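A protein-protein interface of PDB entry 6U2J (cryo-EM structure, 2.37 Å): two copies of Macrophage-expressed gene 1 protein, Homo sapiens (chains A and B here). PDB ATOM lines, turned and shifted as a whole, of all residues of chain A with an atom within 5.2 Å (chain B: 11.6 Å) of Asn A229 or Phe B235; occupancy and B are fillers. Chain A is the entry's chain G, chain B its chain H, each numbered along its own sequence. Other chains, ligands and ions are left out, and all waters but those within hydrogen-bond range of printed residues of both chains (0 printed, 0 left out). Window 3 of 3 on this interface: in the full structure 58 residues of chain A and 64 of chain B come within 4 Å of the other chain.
The backbone carbonyl oxygen of Leu A225 sits at hydrogen-bond distance from the side-chain amide nitrogen of Asn A229.
The side-chain amide oxygen of Asn A232 sits close to the backbone carbonyl oxygen of Gln A228 (2.9 Å).
The side-chain amide oxygen (OD1) of Asn A229 lies within hydrogen-bond range of the side-chain hydroxyl (OG1) of Thr A240.
The side-chain amide nitrogen (ND2) of Asn A229 sits close to the backbone NH (N) of Ser A241 (3.3 Å).
Leu A225 touches Phe B235.
OE1 of Gln A228 touches CD1 of Phe B235 (3.2 Å).
Asn A229 touches Phe B235 (OD1 to CE2, 3.0 Å).
Asn A232 touches Phe B235.
Phe A233 touches Phe B235 (CE2 to CE2, 3.8 Å).
CE1 of Phe A233 touches OE2 of Glu B236 (3.7 Å).
Leu A225 touches just one residue of chain B: Phe B235.
Gln A228 touches one residue of chain B.
Asn A229 touches just one residue of chain B: Phe B235 (3.0 Å).
Val A231 touches none of the printed residues of chain B.
Asn A232 touches just one residue of chain B: Phe B235.
Thr A240 touches none of the printed residues of chain B.
No residue of chain B comes within 4 Å of Ser A241.
Of chain A, only Leu A225 (3.5 Å), Gln A228 (3.2 Å), Asn A229 (3.0 Å), Asn A232 (3.6 Å) and Phe A233 (3.8 Å) come within 4 Å of Phe B235.
Of the printed residues of chain A, Glu B236 touches Phe A233.
Printed residues of chain B that touch a printed residue of chain A: Phe B235 and Glu B236.
Hydrophobic or aromatic side chains of chain B that line the printed part of chain A: Phe B235.
Among the printed residues, 6 pairs touch across the chains.
Among the printed residues, no Asp or Glu carboxylate lies within 4 Å of a Lys or Arg side-chain nitrogen of the other chain.
Positions printed for both chains: 226, 227, 228, 229, 230, 231, 232, 233, 239 and 240.
Of the 6 pairs that touch across the chains among the printed residues, none has its exchanged pair printed and touching as well.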
ATOM      1  N   LEU A 225     -19.795  26.885 -17.391  1.00  0.00           N
ATOM      2  CA  LEU A 225     -21.060  26.548 -18.029  1.00  0.00           C
ATOM      3  C   LEU A 225     -21.101  27.041 -19.468  1.00  0.00           C
ATOM      4  O   LEU A 225     -21.660  26.369 -20.340  1.00  0.00           O
ATOM      5  CB  LEU A 225     -22.218  27.136 -17.225  1.00  0.00           C
ATOM      6  CG  LEU A 225     -23.638  26.854 -17.707  1.00  0.00           C
ATOM      7  CD1 LEU A 225     -23.900  25.383 -17.682  1.00  0.00           C
ATOM      8  CD2 LEU A 225     -24.633  27.565 -16.826  1.00  0.00           C
ATOM      9  N   ALA A 226     -20.509  28.208 -19.731  1.00  0.00           N
ATOM     10  CA  ALA A 226     -20.407  28.710 -21.095  1.00  0.00           C
ATOM     11  C   ALA A 226     -19.498  27.843 -21.951  1.00  0.00           C
ATOM     12  O   ALA A 226     -19.708  27.738 -23.165  1.00  0.00           O
ATOM     13  CB  ALA A 226     -19.895  30.147 -21.089  1.00  0.00           C
ATOM     14  N   PHE A 227     -18.487  27.226 -21.336  1.00  0.00           N
ATOM     15  CA  PHE A 227     -17.618  26.303 -22.055  1.00  0.00           C
ATOM     16  C   PHE A 227     -18.374  25.068 -22.511  1.00  0.00           C
ATOM     17  O   PHE A 227     -18.210  24.623 -23.649  1.00  0.00           O
ATOM     18  CB  PHE A 227     -16.433  25.922 -21.175  1.00  0.00           C
ATOM     19  CG  PHE A 227     -15.573  24.840 -21.740  1.00  0.00           C
ATOM     20  CD1 PHE A 227     -14.894  25.019 -22.929  1.00  0.00           C
ATOM     21  CD2 PHE A 227     -15.388  23.667 -21.042  1.00  0.00           C
ATOM     22  CE1 PHE A 227     -14.086  24.026 -23.439  1.00  0.00           C
ATOM     23  CE2 PHE A 227     -14.578  22.676 -21.536  1.00  0.00           C
ATOM     24  CZ  PHE A 227     -13.927  22.853 -22.736  1.00  0.00           C
ATOM     25  N   GLN A 228     -19.228  24.520 -21.655  1.00  0.00           N
ATOM     26  CA  GLN A 228     -19.994  23.358 -22.064  1.00  0.00           C
ATOM     27  C   GLN A 228     -21.123  23.708 -23.022  1.00  0.00           C
ATOM     28  O   GLN A 228     -21.567  22.834 -23.766  1.00  0.00           O
ATOM     29  CB  GLN A 228     -20.522  22.616 -20.840  1.00  0.00           C
ATOM     30  CG  GLN A 228     -19.415  22.036 -19.995  1.00  0.00           C
ATOM     31  CD  GLN A 228     -19.913  21.191 -18.847  1.00  0.00           C
ATOM     32  OE1 GLN A 228     -21.107  20.976 -18.696  1.00  0.00           O
ATOM     33  NE2 GLN A 228     -19.001  20.735 -18.013  1.00  0.00           N
ATOM     34  N   ASN A 229     -21.569  24.965 -23.046  1.00  0.00           N
ATOM     35  CA  ASN A 229     -22.496  25.392 -24.090  1.00  0.00           C
ATOM     36  C   ASN A 229     -21.799  25.520 -25.434  1.00  0.00           C
ATOM     37  O   ASN A 229     -22.387  25.200 -26.473  1.00  0.00           O
ATOM     38  CB  ASN A 229     -23.146  26.725 -23.727  1.00  0.00           C
ATOM     39  CG  ASN A 229     -24.244  26.582 -22.708  1.00  0.00           C
ATOM     40  OD1 ASN A 229     -25.060  25.673 -22.782  1.00  0.00           O
ATOM     41  ND2 ASN A 229     -24.287  27.499 -21.764  1.00  0.00           N
ATOM     42  N   THR A 230     -20.555  26.009 -25.430  1.00  0.00           N
ATOM     43  CA  THR A 230     -19.805  26.197 -26.666  1.00  0.00           C
ATOM     44  C   THR A 230     -19.509  24.867 -27.336  1.00  0.00           C
ATOM     45  O   THR A 230     -19.661  24.735 -28.554  1.00  0.00           O
ATOM     46  CB  THR A 230     -18.510  26.954 -26.383  1.00  0.00           C
ATOM     47  OG1 THR A 230     -18.816  28.221 -25.797  1.00  0.00           O
ATOM     48  CG2 THR A 230     -17.731  27.189 -27.655  1.00  0.00           C
ATOM     49  N   VAL A 231     -19.123  23.857 -26.556  1.00  0.00           N
ATOM     50  CA  VAL A 231     -18.846  22.560 -27.153  1.00  0.00           C
ATOM     51  C   VAL A 231     -20.146  21.881 -27.588  1.00  0.00           C
ATOM     52  O   VAL A 231     -20.328  21.620 -28.775  1.00  0.00           O
ATOM     53  CB  VAL A 231     -17.948  21.701 -26.229  1.00  0.00           C
ATOM     54  CG1 VAL A 231     -18.475  21.537 -24.847  1.00  0.00           C
ATOM     55  CG2 VAL A 231     -17.699  20.342 -26.816  1.00  0.00           C
ATOM     56  N   ASN A 232     -21.133  21.756 -26.695  1.00  0.00           N
ATOM     57  CA  ASN A 232     -22.288  20.903 -26.984  1.00  0.00           C
ATOM     58  C   ASN A 232     -23.253  21.508 -27.998  1.00  0.00           C
ATOM     59  O   ASN A 232     -23.804  20.780 -28.828  1.00  0.00           O
ATOM     60  CB  ASN A 232     -23.038  20.563 -25.698  1.00  0.00           C
ATOM     61  CG  ASN A 232     -22.277  19.596 -24.825  1.00  0.00           C
ATOM     62  OD1 ASN A 232     -21.865  19.927 -23.721  1.00  0.00           O
ATOM     63  ND2 ASN A 232     -22.084  18.385 -25.323  1.00  0.00           N
ATOM     64  N   PHE A 233     -23.473  22.814 -27.965  1.00  0.00           N
ATOM     65  CA  PHE A 233     -24.442  23.397 -28.878  1.00  0.00           C
ATOM     66  C   PHE A 233     -23.776  23.911 -30.140  1.00  0.00           C
ATOM     67  O   PHE A 233     -22.606  24.301 -30.145  1.00  0.00           O
ATOM     68  CB  PHE A 233     -25.226  24.529 -28.222  1.00  0.00           C
ATOM     69  CG  PHE A 233     -26.154  24.065 -27.157  1.00  0.00           C
ATOM     70  CD1 PHE A 233     -27.300  23.368 -27.491  1.00  0.00           C
ATOM     71  CD2 PHE A 233     -25.899  24.340 -25.829  1.00  0.00           C
ATOM     72  CE1 PHE A 233     -28.162  22.932 -26.516  1.00  0.00           C
ATOM     73  CE2 PHE A 233     -26.760  23.912 -24.851  1.00  0.00           C
ATOM     74  CZ  PHE A 233     -27.893  23.209 -25.192  1.00  0.00           C
ATOM     75  N   TYR A 239     -28.030  28.653 -26.115  1.00  0.00           N
ATOM     76  CA  TYR A 239     -27.292  28.410 -24.888  1.00  0.00           C
ATOM     77  C   TYR A 239     -28.205  28.524 -23.672  1.00  0.00           C
ATOM     78  O   TYR A 239     -29.312  29.063 -23.735  1.00  0.00           O
ATOM     79  CB  TYR A 239     -26.119  29.385 -24.744  1.00  0.00           C
ATOM     80  CG  TYR A 239     -24.990  29.213 -25.745  1.00  0.00           C
ATOM     81  CD1 TYR A 239     -24.927  28.107 -26.587  1.00  0.00           C
ATOM     82  CD2 TYR A 239     -23.968  30.150 -25.824  1.00  0.00           C
ATOM     83  CE1 TYR A 239     -23.899  27.957 -27.492  1.00  0.00           C
ATOM     84  CE2 TYR A 239     -22.931  30.001 -26.723  1.00  0.00           C
ATOM     85  CZ  TYR A 239     -22.904  28.905 -27.553  1.00  0.00           C
ATOM     86  OH  TYR A 239     -21.873  28.756 -28.450  1.00  0.00           O
ATOM     87  N   THR A 240     -27.718  28.003 -22.546  1.00  0.00           N
ATOM     88  CA  THR A 240     -28.455  28.021 -21.292  1.00  0.00           C
ATOM     89  C   THR A 240     -27.785  28.858 -20.211  1.00  0.00           C
ATOM     90  O   THR A 240     -28.341  28.979 -19.112  1.00  0.00           O
ATOM     91  CB  THR A 240     -28.655  26.591 -20.773  1.00  0.00           C
ATOM     92  OG1 THR A 240     -27.380  26.003 -20.492  1.00  0.00           O
ATOM     93  CG2 THR A 240     -29.375  25.742 -21.808  1.00  0.00           C
ATOM     94  N   SER A 241     -26.617  29.444 -20.484  1.00  0.00           N
ATOM     95  CA  SER A 241     -25.902  30.271 -19.518  1.00  0.00           C
ATOM     96  C   SER A 241     -26.205  31.754 -19.692  1.00  0.00           C
ATOM     97  O   SER A 241     -25.343  32.599 -19.434  1.00  0.00           O
ATOM     98  CB  SER A 241     -24.398  30.032 -19.616  1.00  0.00           C
ATOM     99  OG  SER A 241     -23.697  30.848 -18.698  1.00  0.00           O
ATOM    100  N   ALA B 226     -27.053  15.014  -6.885  1.00  0.00           N
ATOM    101  CA  ALA B 226     -26.566  15.837  -7.987  1.00  0.00           C
ATOM    102  C   ALA B 226     -25.533  15.102  -8.827  1.00  0.00           C
ATOM    103  O   ALA B 226     -25.430  15.349 -10.033  1.00  0.00           O
ATOM    104  CB  ALA B 226     -25.967  17.132  -7.449  1.00  0.00           C
ATOM    105  N   PHE B 227     -24.765  14.207  -8.204  1.00  0.00           N
ATOM    106  CA  PHE B 227     -23.811  13.389  -8.941  1.00  0.00           C
ATOM    107  C   PHE B 227     -24.513  12.439  -9.894  1.00  0.00           C
ATOM    108  O   PHE B 227     -24.095  12.288 -11.044  1.00  0.00           O
ATOM    109  CB  PHE B 227     -22.925  12.625  -7.964  1.00  0.00           C
ATOM    110  CG  PHE B 227     -22.031  11.616  -8.607  1.00  0.00           C
ATOM    111  CD1 PHE B 227     -21.058  11.999  -9.507  1.00  0.00           C
ATOM    112  CD2 PHE B 227     -22.122  10.287  -8.254  1.00  0.00           C
ATOM    113  CE1 PHE B 227     -20.221  11.069 -10.085  1.00  0.00           C
ATOM    114  CE2 PHE B 227     -21.288   9.353  -8.817  1.00  0.00           C
ATOM    115  CZ  PHE B 227     -20.337   9.743  -9.735  1.00  0.00           C
ATOM    116  N   GLN B 228     -25.597  11.814  -9.450  1.00  0.00           N
ATOM    117  CA  GLN B 228     -26.316  10.922 -10.341  1.00  0.00           C
ATOM    118  C   GLN B 228     -27.131  11.669 -11.386  1.00  0.00           C
ATOM    119  O   GLN B 228     -27.432  11.095 -12.432  1.00  0.00           O
ATOM    120  CB  GLN B 228     -27.196   9.970  -9.536  1.00  0.00           C
ATOM    121  CG  GLN B 228     -26.392   9.037  -8.666  1.00  0.00           C
ATOM    122  CD  GLN B 228     -27.231   8.000  -7.957  1.00  0.00           C
ATOM    123  OE1 GLN B 228     -28.436   7.928  -8.149  1.00  0.00           O
ATOM    124  NE2 GLN B 228     -26.602   7.217  -7.105  1.00  0.00           N
ATOM    125  N   ASN B 229     -27.461  12.939 -11.148  1.00  0.00           N
ATOM    126  CA  ASN B 229     -28.052  13.753 -12.205  1.00  0.00           C
ATOM    127  C   ASN B 229     -27.023  14.127 -13.261  1.00  0.00           C
ATOM    128  O   ASN B 229     -27.346  14.178 -14.451  1.00  0.00           O
ATOM    129  CB  ASN B 229     -28.672  15.024 -11.629  1.00  0.00           C
ATOM    130  CG  ASN B 229     -30.004  14.780 -10.972  1.00  0.00           C
ATOM    131  OD1 ASN B 229     -30.838  14.049 -11.489  1.00  0.00           O
ATOM    132  ND2 ASN B 229     -30.221  15.413  -9.840  1.00  0.00           N
ATOM    133  N   THR B 230     -25.791  14.413 -12.832  1.00  0.00           N
ATOM    134  CA  THR B 230     -24.736  14.808 -13.758  1.00  0.00           C
ATOM    135  C   THR B 230     -24.376  13.671 -14.697  1.00  0.00           C
ATOM    136  O   THR B 230     -24.218  13.885 -15.903  1.00  0.00           O
ATOM    137  CB  THR B 230     -23.504  15.269 -12.981  1.00  0.00           C
ATOM    138  OG1 THR B 230     -23.856  16.370 -12.140  1.00  0.00           O
ATOM    139  CG2 THR B 230     -22.408  15.714 -13.919  1.00  0.00           C
ATOM    140  N   VAL B 231     -24.281  12.448 -14.177  1.00  0.00           N
ATOM    141  CA  VAL B 231     -23.957  11.325 -15.044  1.00  0.00           C
ATOM    142  C   VAL B 231     -25.148  10.979 -15.939  1.00  0.00           C
ATOM    143  O   VAL B 231     -25.036  11.066 -17.159  1.00  0.00           O
ATOM    144  CB  VAL B 231     -23.394  10.134 -14.229  1.00  0.00           C
ATOM    145  CG1 VAL B 231     -24.271   9.694 -13.110  1.00  0.00           C
ATOM    146  CG2 VAL B 231     -23.104   8.956 -15.110  1.00  0.00           C
ATOM    147  N   ASN B 232     -26.338  10.768 -15.368  1.00  0.00           N
ATOM    148  CA  ASN B 232     -27.438  10.196 -16.145  1.00  0.00           C
ATOM    149  C   ASN B 232     -28.061  11.177 -17.133  1.00  0.00           C
ATOM    150  O   ASN B 232     -28.432  10.779 -18.241  1.00  0.00           O
ATOM    151  CB  ASN B 232     -28.519   9.644 -15.219  1.00  0.00           C
ATOM    152  CG  ASN B 232     -28.083   8.381 -14.514  1.00  0.00           C
ATOM    153  OD1 ASN B 232     -27.947   8.350 -13.297  1.00  0.00           O
ATOM    154  ND2 ASN B 232     -27.860   7.328 -15.283  1.00  0.00           N
ATOM    155  N   PHE B 233     -28.184  12.447 -16.776  1.00  0.00           N
ATOM    156  CA  PHE B 233     -28.838  13.381 -17.676  1.00  0.00           C
ATOM    157  C   PHE B 233     -27.833  14.106 -18.551  1.00  0.00           C
ATOM    158  O   PHE B 233     -26.677  14.310 -18.177  1.00  0.00           O
ATOM    159  CB  PHE B 233     -29.678  14.403 -16.918  1.00  0.00           C
ATOM    160  CG  PHE B 233     -30.882  13.815 -16.272  1.00  0.00           C
ATOM    161  CD1 PHE B 233     -31.951  13.403 -17.042  1.00  0.00           C
ATOM    162  CD2 PHE B 233     -30.960  13.694 -14.898  1.00  0.00           C
ATOM    163  CE1 PHE B 233     -33.067  12.856 -16.457  1.00  0.00           C
ATOM    164  CE2 PHE B 233     -32.073  13.154 -14.307  1.00  0.00           C
ATOM    165  CZ  PHE B 233     -33.129  12.735 -15.086  1.00  0.00           C
ATOM    166  N   LYS B 234     -28.305  14.517 -19.721  1.00  0.00           N
ATOM    167  CA  LYS B 234     -27.497  15.287 -20.648  1.00  0.00           C
ATOM    168  C   LYS B 234     -27.235  16.683 -20.089  1.00  0.00           C
ATOM    169  O   LYS B 234     -27.798  17.100 -19.073  1.00  0.00           O
ATOM    170  CB  LYS B 234     -28.191  15.371 -22.002  1.00  0.00           C
ATOM    171  CG  LYS B 234     -28.395  14.036 -22.680  1.00  0.00           C
ATOM    172  CD  LYS B 234     -27.064  13.390 -22.994  1.00  0.00           C
ATOM    173  CE  LYS B 234     -26.316  14.142 -24.073  1.00  0.00           C
ATOM    174  NZ  LYS B 234     -25.033  13.473 -24.409  1.00  0.00           N
ATOM    175  N   PHE B 235     -26.371  17.419 -20.788  1.00  0.00           N
ATOM    176  CA  PHE B 235     -25.984  18.756 -20.350  1.00  0.00           C
ATOM    177  C   PHE B 235     -27.159  19.737 -20.374  1.00  0.00           C
ATOM    178  O   PHE B 235     -27.173  20.703 -19.600  1.00  0.00           O
ATOM    179  CB  PHE B 235     -24.808  19.237 -21.203  1.00  0.00           C
ATOM    180  CG  PHE B 235     -24.509  20.685 -21.055  1.00  0.00           C
ATOM    181  CD1 PHE B 235     -24.062  21.196 -19.849  1.00  0.00           C
ATOM    182  CD2 PHE B 235     -24.663  21.538 -22.133  1.00  0.00           C
ATOM    183  CE1 PHE B 235     -23.808  22.533 -19.713  1.00  0.00           C
ATOM    184  CE2 PHE B 235     -24.395  22.873 -22.007  1.00  0.00           C
ATOM    185  CZ  PHE B 235     -23.964  23.377 -20.798  1.00  0.00           C
ATOM    186  N   GLU B 236     -28.167  19.483 -21.207  1.00  0.00           N
ATOM    187  CA  GLU B 236     -29.427  20.206 -21.104  1.00  0.00           C
ATOM    188  C   GLU B 236     -30.084  19.914 -19.757  1.00  0.00           C
ATOM    189  O   GLU B 236     -30.224  18.753 -19.357  1.00  0.00           O
ATOM    190  CB  GLU B 236     -30.358  19.815 -22.250  1.00  0.00           C
ATOM    191  CG  GLU B 236     -29.852  20.229 -23.623  1.00  0.00           C
ATOM    192  CD  GLU B 236     -28.941  19.194 -24.246  1.00  0.00           C
ATOM    193  OE1 GLU B 236     -28.795  18.112 -23.655  1.00  0.00           O
ATOM    194  OE2 GLU B 236     -28.365  19.460 -25.319  1.00  0.00           O
ATOM    195  N   GLU B 237     -30.466  20.978 -19.053  1.00  0.00           N
ATOM    196  CA  GLU B 237     -30.818  20.892 -17.639  1.00  0.00           C
ATOM    197  C   GLU B 237     -32.180  20.236 -17.460  1.00  0.00           C
ATOM    198  O   GLU B 237     -33.219  20.845 -17.734  1.00  0.00           O
ATOM    199  CB  GLU B 237     -30.798  22.284 -17.014  1.00  0.00           C
ATOM    200  CG  GLU B 237     -31.161  22.308 -15.545  1.00  0.00           C
ATOM    201  CD  GLU B 237     -30.139  21.619 -14.667  1.00  0.00           C
ATOM    202  OE1 GLU B 237     -28.946  21.583 -15.032  1.00  0.00           O
ATOM    203  OE2 GLU B 237     -30.537  21.113 -13.599  1.00  0.00           O
ATOM    204  N   ASN B 238     -32.170  18.994 -16.983  1.00  0.00           N
ATOM    205  CA  ASN B 238     -33.377  18.226 -16.707  1.00  0.00           C
ATOM    206  C   ASN B 238     -33.246  17.525 -15.364  1.00  0.00           C
ATOM    207  O   ASN B 238     -33.706  16.394 -15.185  1.00  0.00           O
ATOM    208  CB  ASN B 238     -33.646  17.216 -17.819  1.00  0.00           C
ATOM    209  CG  ASN B 238     -34.009  17.878 -19.129  1.00  0.00           C
ATOM    210  OD1 ASN B 238     -34.796  18.825 -19.161  1.00  0.00           O
ATOM    211  ND2 ASN B 238     -33.425  17.394 -20.217  1.00  0.00           N
ATOM    212  N   TYR B 239     -32.617  18.192 -14.402  1.00  0.00           N
ATOM    213  CA  TYR B 239     -32.240  17.532 -13.164  1.00  0.00           C
ATOM    214  C   TYR B 239     -33.425  17.455 -12.206  1.00  0.00           C
ATOM    215  O   TYR B 239     -34.435  18.146 -12.361  1.00  0.00           O
ATOM    216  CB  TYR B 239     -31.075  18.257 -12.481  1.00  0.00           C
ATOM    217  CG  TYR B 239     -29.742  18.192 -13.206  1.00  0.00           C
ATOM    218  CD1 TYR B 239     -29.546  17.348 -14.294  1.00  0.00           C
ATOM    219  CD2 TYR B 239     -28.668  18.959 -12.777  1.00  0.00           C
ATOM    220  CE1 TYR B 239     -28.333  17.294 -14.947  1.00  0.00           C
ATOM    221  CE2 TYR B 239     -27.447  18.904 -13.421  1.00  0.00           C
ATOM    222  CZ  TYR B 239     -27.288  18.070 -14.503  1.00  0.00           C
ATOM    223  OH  TYR B 239     -26.075  18.014 -15.147  1.00  0.00           O
ATOM    224  N   THR B 240     -33.286  16.594 -11.200  1.00  0.00           N
ATOM    225  CA  THR B 240     -34.318  16.389 -10.196  1.00  0.00           C
ATOM    226  C   THR B 240     -33.890  16.809  -8.796  1.00  0.00           C
ATOM    227  O   THR B 240     -34.700  16.716  -7.865  1.00  0.00           O
ATOM    228  CB  THR B 240     -34.751  14.918 -10.171  1.00  0.00           C
ATOM    229  OG1 THR B 240     -33.640  14.099  -9.790  1.00  0.00           O
ATOM    230  CG2 THR B 240     -35.241  14.481 -11.542  1.00  0.00           C
ATOM    231  N   GLN B 242     -33.317  19.812  -7.703  1.00  0.00           N
ATOM    232  CA  GLN B 242     -33.552  21.246  -7.618  1.00  0.00           C
ATOM    233  C   GLN B 242     -34.637  21.502  -6.578  1.00  0.00           C
ATOM    234  O   GLN B 242     -35.815  21.222  -6.818  1.00  0.00           O
ATOM    235  CB  GLN B 242     -33.953  21.802  -8.980  1.00  0.00           C
ATOM    236  CG  GLN B 242     -32.868  21.687 -10.029  1.00  0.00           C
ATOM    237  CD  GLN B 242     -33.301  22.241 -11.369  1.00  0.00           C
ATOM    238  OE1 GLN B 242     -34.441  22.673 -11.535  1.00  0.00           O
ATOM    239  NE2 GLN B 242     -32.394  22.225 -12.337  1.00  0.00           N
ATOM    240  N   VAL B 258     -15.427  16.454 -12.108  1.00  0.00           N
ATOM    241  CA  VAL B 258     -15.734  15.036 -12.204  1.00  0.00           C
ATOM    242  C   VAL B 258     -14.543  14.371 -12.862  1.00  0.00           C
ATOM    243  O   VAL B 258     -14.138  14.774 -13.956  1.00  0.00           O
ATOM    244  CB  VAL B 258     -17.008  14.778 -13.019  1.00  0.00           C
ATOM    245  CG1 VAL B 258     -17.235  13.296 -13.178  1.00  0.00           C
ATOM    246  CG2 VAL B 258     -18.199  15.425 -12.370  1.00  0.00           C
ATOM    247  N   PHE B 266     -15.308   9.992 -19.399  1.00  0.00           N
ATOM    248  CA  PHE B 266     -16.594  10.488 -18.946  1.00  0.00           C
ATOM    249  C   PHE B 266     -17.027  11.704 -19.754  1.00  0.00           C
ATOM    250  O   PHE B 266     -16.212  12.545 -20.132  1.00  0.00           O
ATOM    251  CB  PHE B 266     -16.534  10.852 -17.462  1.00  0.00           C
ATOM    252  CG  PHE B 266     -17.817  11.409 -16.928  1.00  0.00           C
ATOM    253  CD1 PHE B 266     -18.890  10.579 -16.676  1.00  0.00           C
ATOM    254  CD2 PHE B 266     -17.960  12.767 -16.706  1.00  0.00           C
ATOM    255  CE1 PHE B 266     -20.075  11.089 -16.202  1.00  0.00           C
ATOM    256  CE2 PHE B 266     -19.145  13.279 -16.239  1.00  0.00           C
ATOM    257  CZ  PHE B 266     -20.201  12.439 -15.983  1.00  0.00           C
ATOM    258  N   TYR B 267     -18.326  11.788 -20.009  1.00  0.00           N
ATOM    259  CA  TYR B 267     -18.990  12.996 -20.456  1.00  0.00           C
ATOM    260  C   TYR B 267     -20.338  13.055 -19.761  1.00  0.00           C
ATOM    261  O   TYR B 267     -20.920  12.010 -19.460  1.00  0.00           O
ATOM    262  CB  TYR B 267     -19.154  13.035 -21.984  1.00  0.00           C
ATOM    263  CG  TYR B 267     -19.893  11.871 -22.587  1.00  0.00           C
ATOM    264  CD1 TYR B 267     -19.216  10.722 -22.962  1.00  0.00           C
ATOM    265  CD2 TYR B 267     -21.257  11.928 -22.812  1.00  0.00           C
ATOM    266  CE1 TYR B 267     -19.877   9.660 -23.519  1.00  0.00           C
ATOM    267  CE2 TYR B 267     -21.926  10.868 -23.369  1.00  0.00           C
ATOM    268  CZ  TYR B 267     -21.230   9.741 -23.721  1.00  0.00           C
ATOM    269  OH  TYR B 267     -21.892   8.682 -24.280  1.00  0.00           O
ATOM    270  N   PRO B 268     -20.837  14.253 -19.452  1.00  0.00           N
ATOM    271  CA  PRO B 268     -22.158  14.353 -18.822  1.00  0.00           C
ATOM    272  C   PRO B 268     -23.269  13.882 -19.739  1.00  0.00           C
ATOM    273  O   PRO B 268     -23.526  14.491 -20.777  1.00  0.00           O
ATOM    274  CB  PRO B 268     -22.285  15.848 -18.516  1.00  0.00           C
ATOM    275  CG  PRO B 268     -20.907  16.334 -18.465  1.00  0.00           C
ATOM    276  CD  PRO B 268     -20.161  15.556 -19.483  1.00  0.00           C
ATOM    277  N   GLY B 269     -23.918  12.788 -19.372  1.00  0.00           N
ATOM    278  CA  GLY B 269     -24.948  12.237 -20.219  1.00  0.00           C
ATOM    279  C   GLY B 269     -24.745  10.779 -20.557  1.00  0.00           C
ATOM    280  O   GLY B 269     -25.675  10.127 -21.033  1.00  0.00           O
ATOM    281  N   ILE B 270     -23.531  10.264 -20.357  1.00  0.00           N
ATOM    282  CA  ILE B 270     -23.320   8.826 -20.423  1.00  0.00           C
ATOM    283  C   ILE B 270     -24.082   8.193 -19.271  1.00  0.00           C
ATOM    284  O   ILE B 270     -24.137   8.741 -18.171  1.00  0.00           O
ATOM    285  CB  ILE B 270     -21.810   8.491 -20.402  1.00  0.00           C
ATOM    286  CG1 ILE B 270     -21.553   7.037 -20.757  1.00  0.00           C
ATOM    287  CG2 ILE B 270     -21.129   8.785 -19.071  1.00  0.00           C
ATOM    288  CD1 ILE B 270     -20.098   6.747 -20.976  1.00  0.00           C
ATOM    289  N   THR B 271     -24.770   7.100 -19.524  1.00  0.00           N
ATOM    290  CA  THR B 271     -25.502   6.600 -18.373  1.00  0.00           C
ATOM    291  C   THR B 271     -24.567   5.799 -17.476  1.00  0.00           C
ATOM    292  O   THR B 271     -23.456   5.436 -17.866  1.00  0.00           O
ATOM    293  CB  THR B 271     -26.709   5.784 -18.814  1.00  0.00           C
ATOM    294  OG1 THR B 271     -26.288   4.723 -19.674  1.00  0.00           O
ATOM    295  CG2 THR B 271     -27.684   6.679 -19.552  1.00  0.00           C
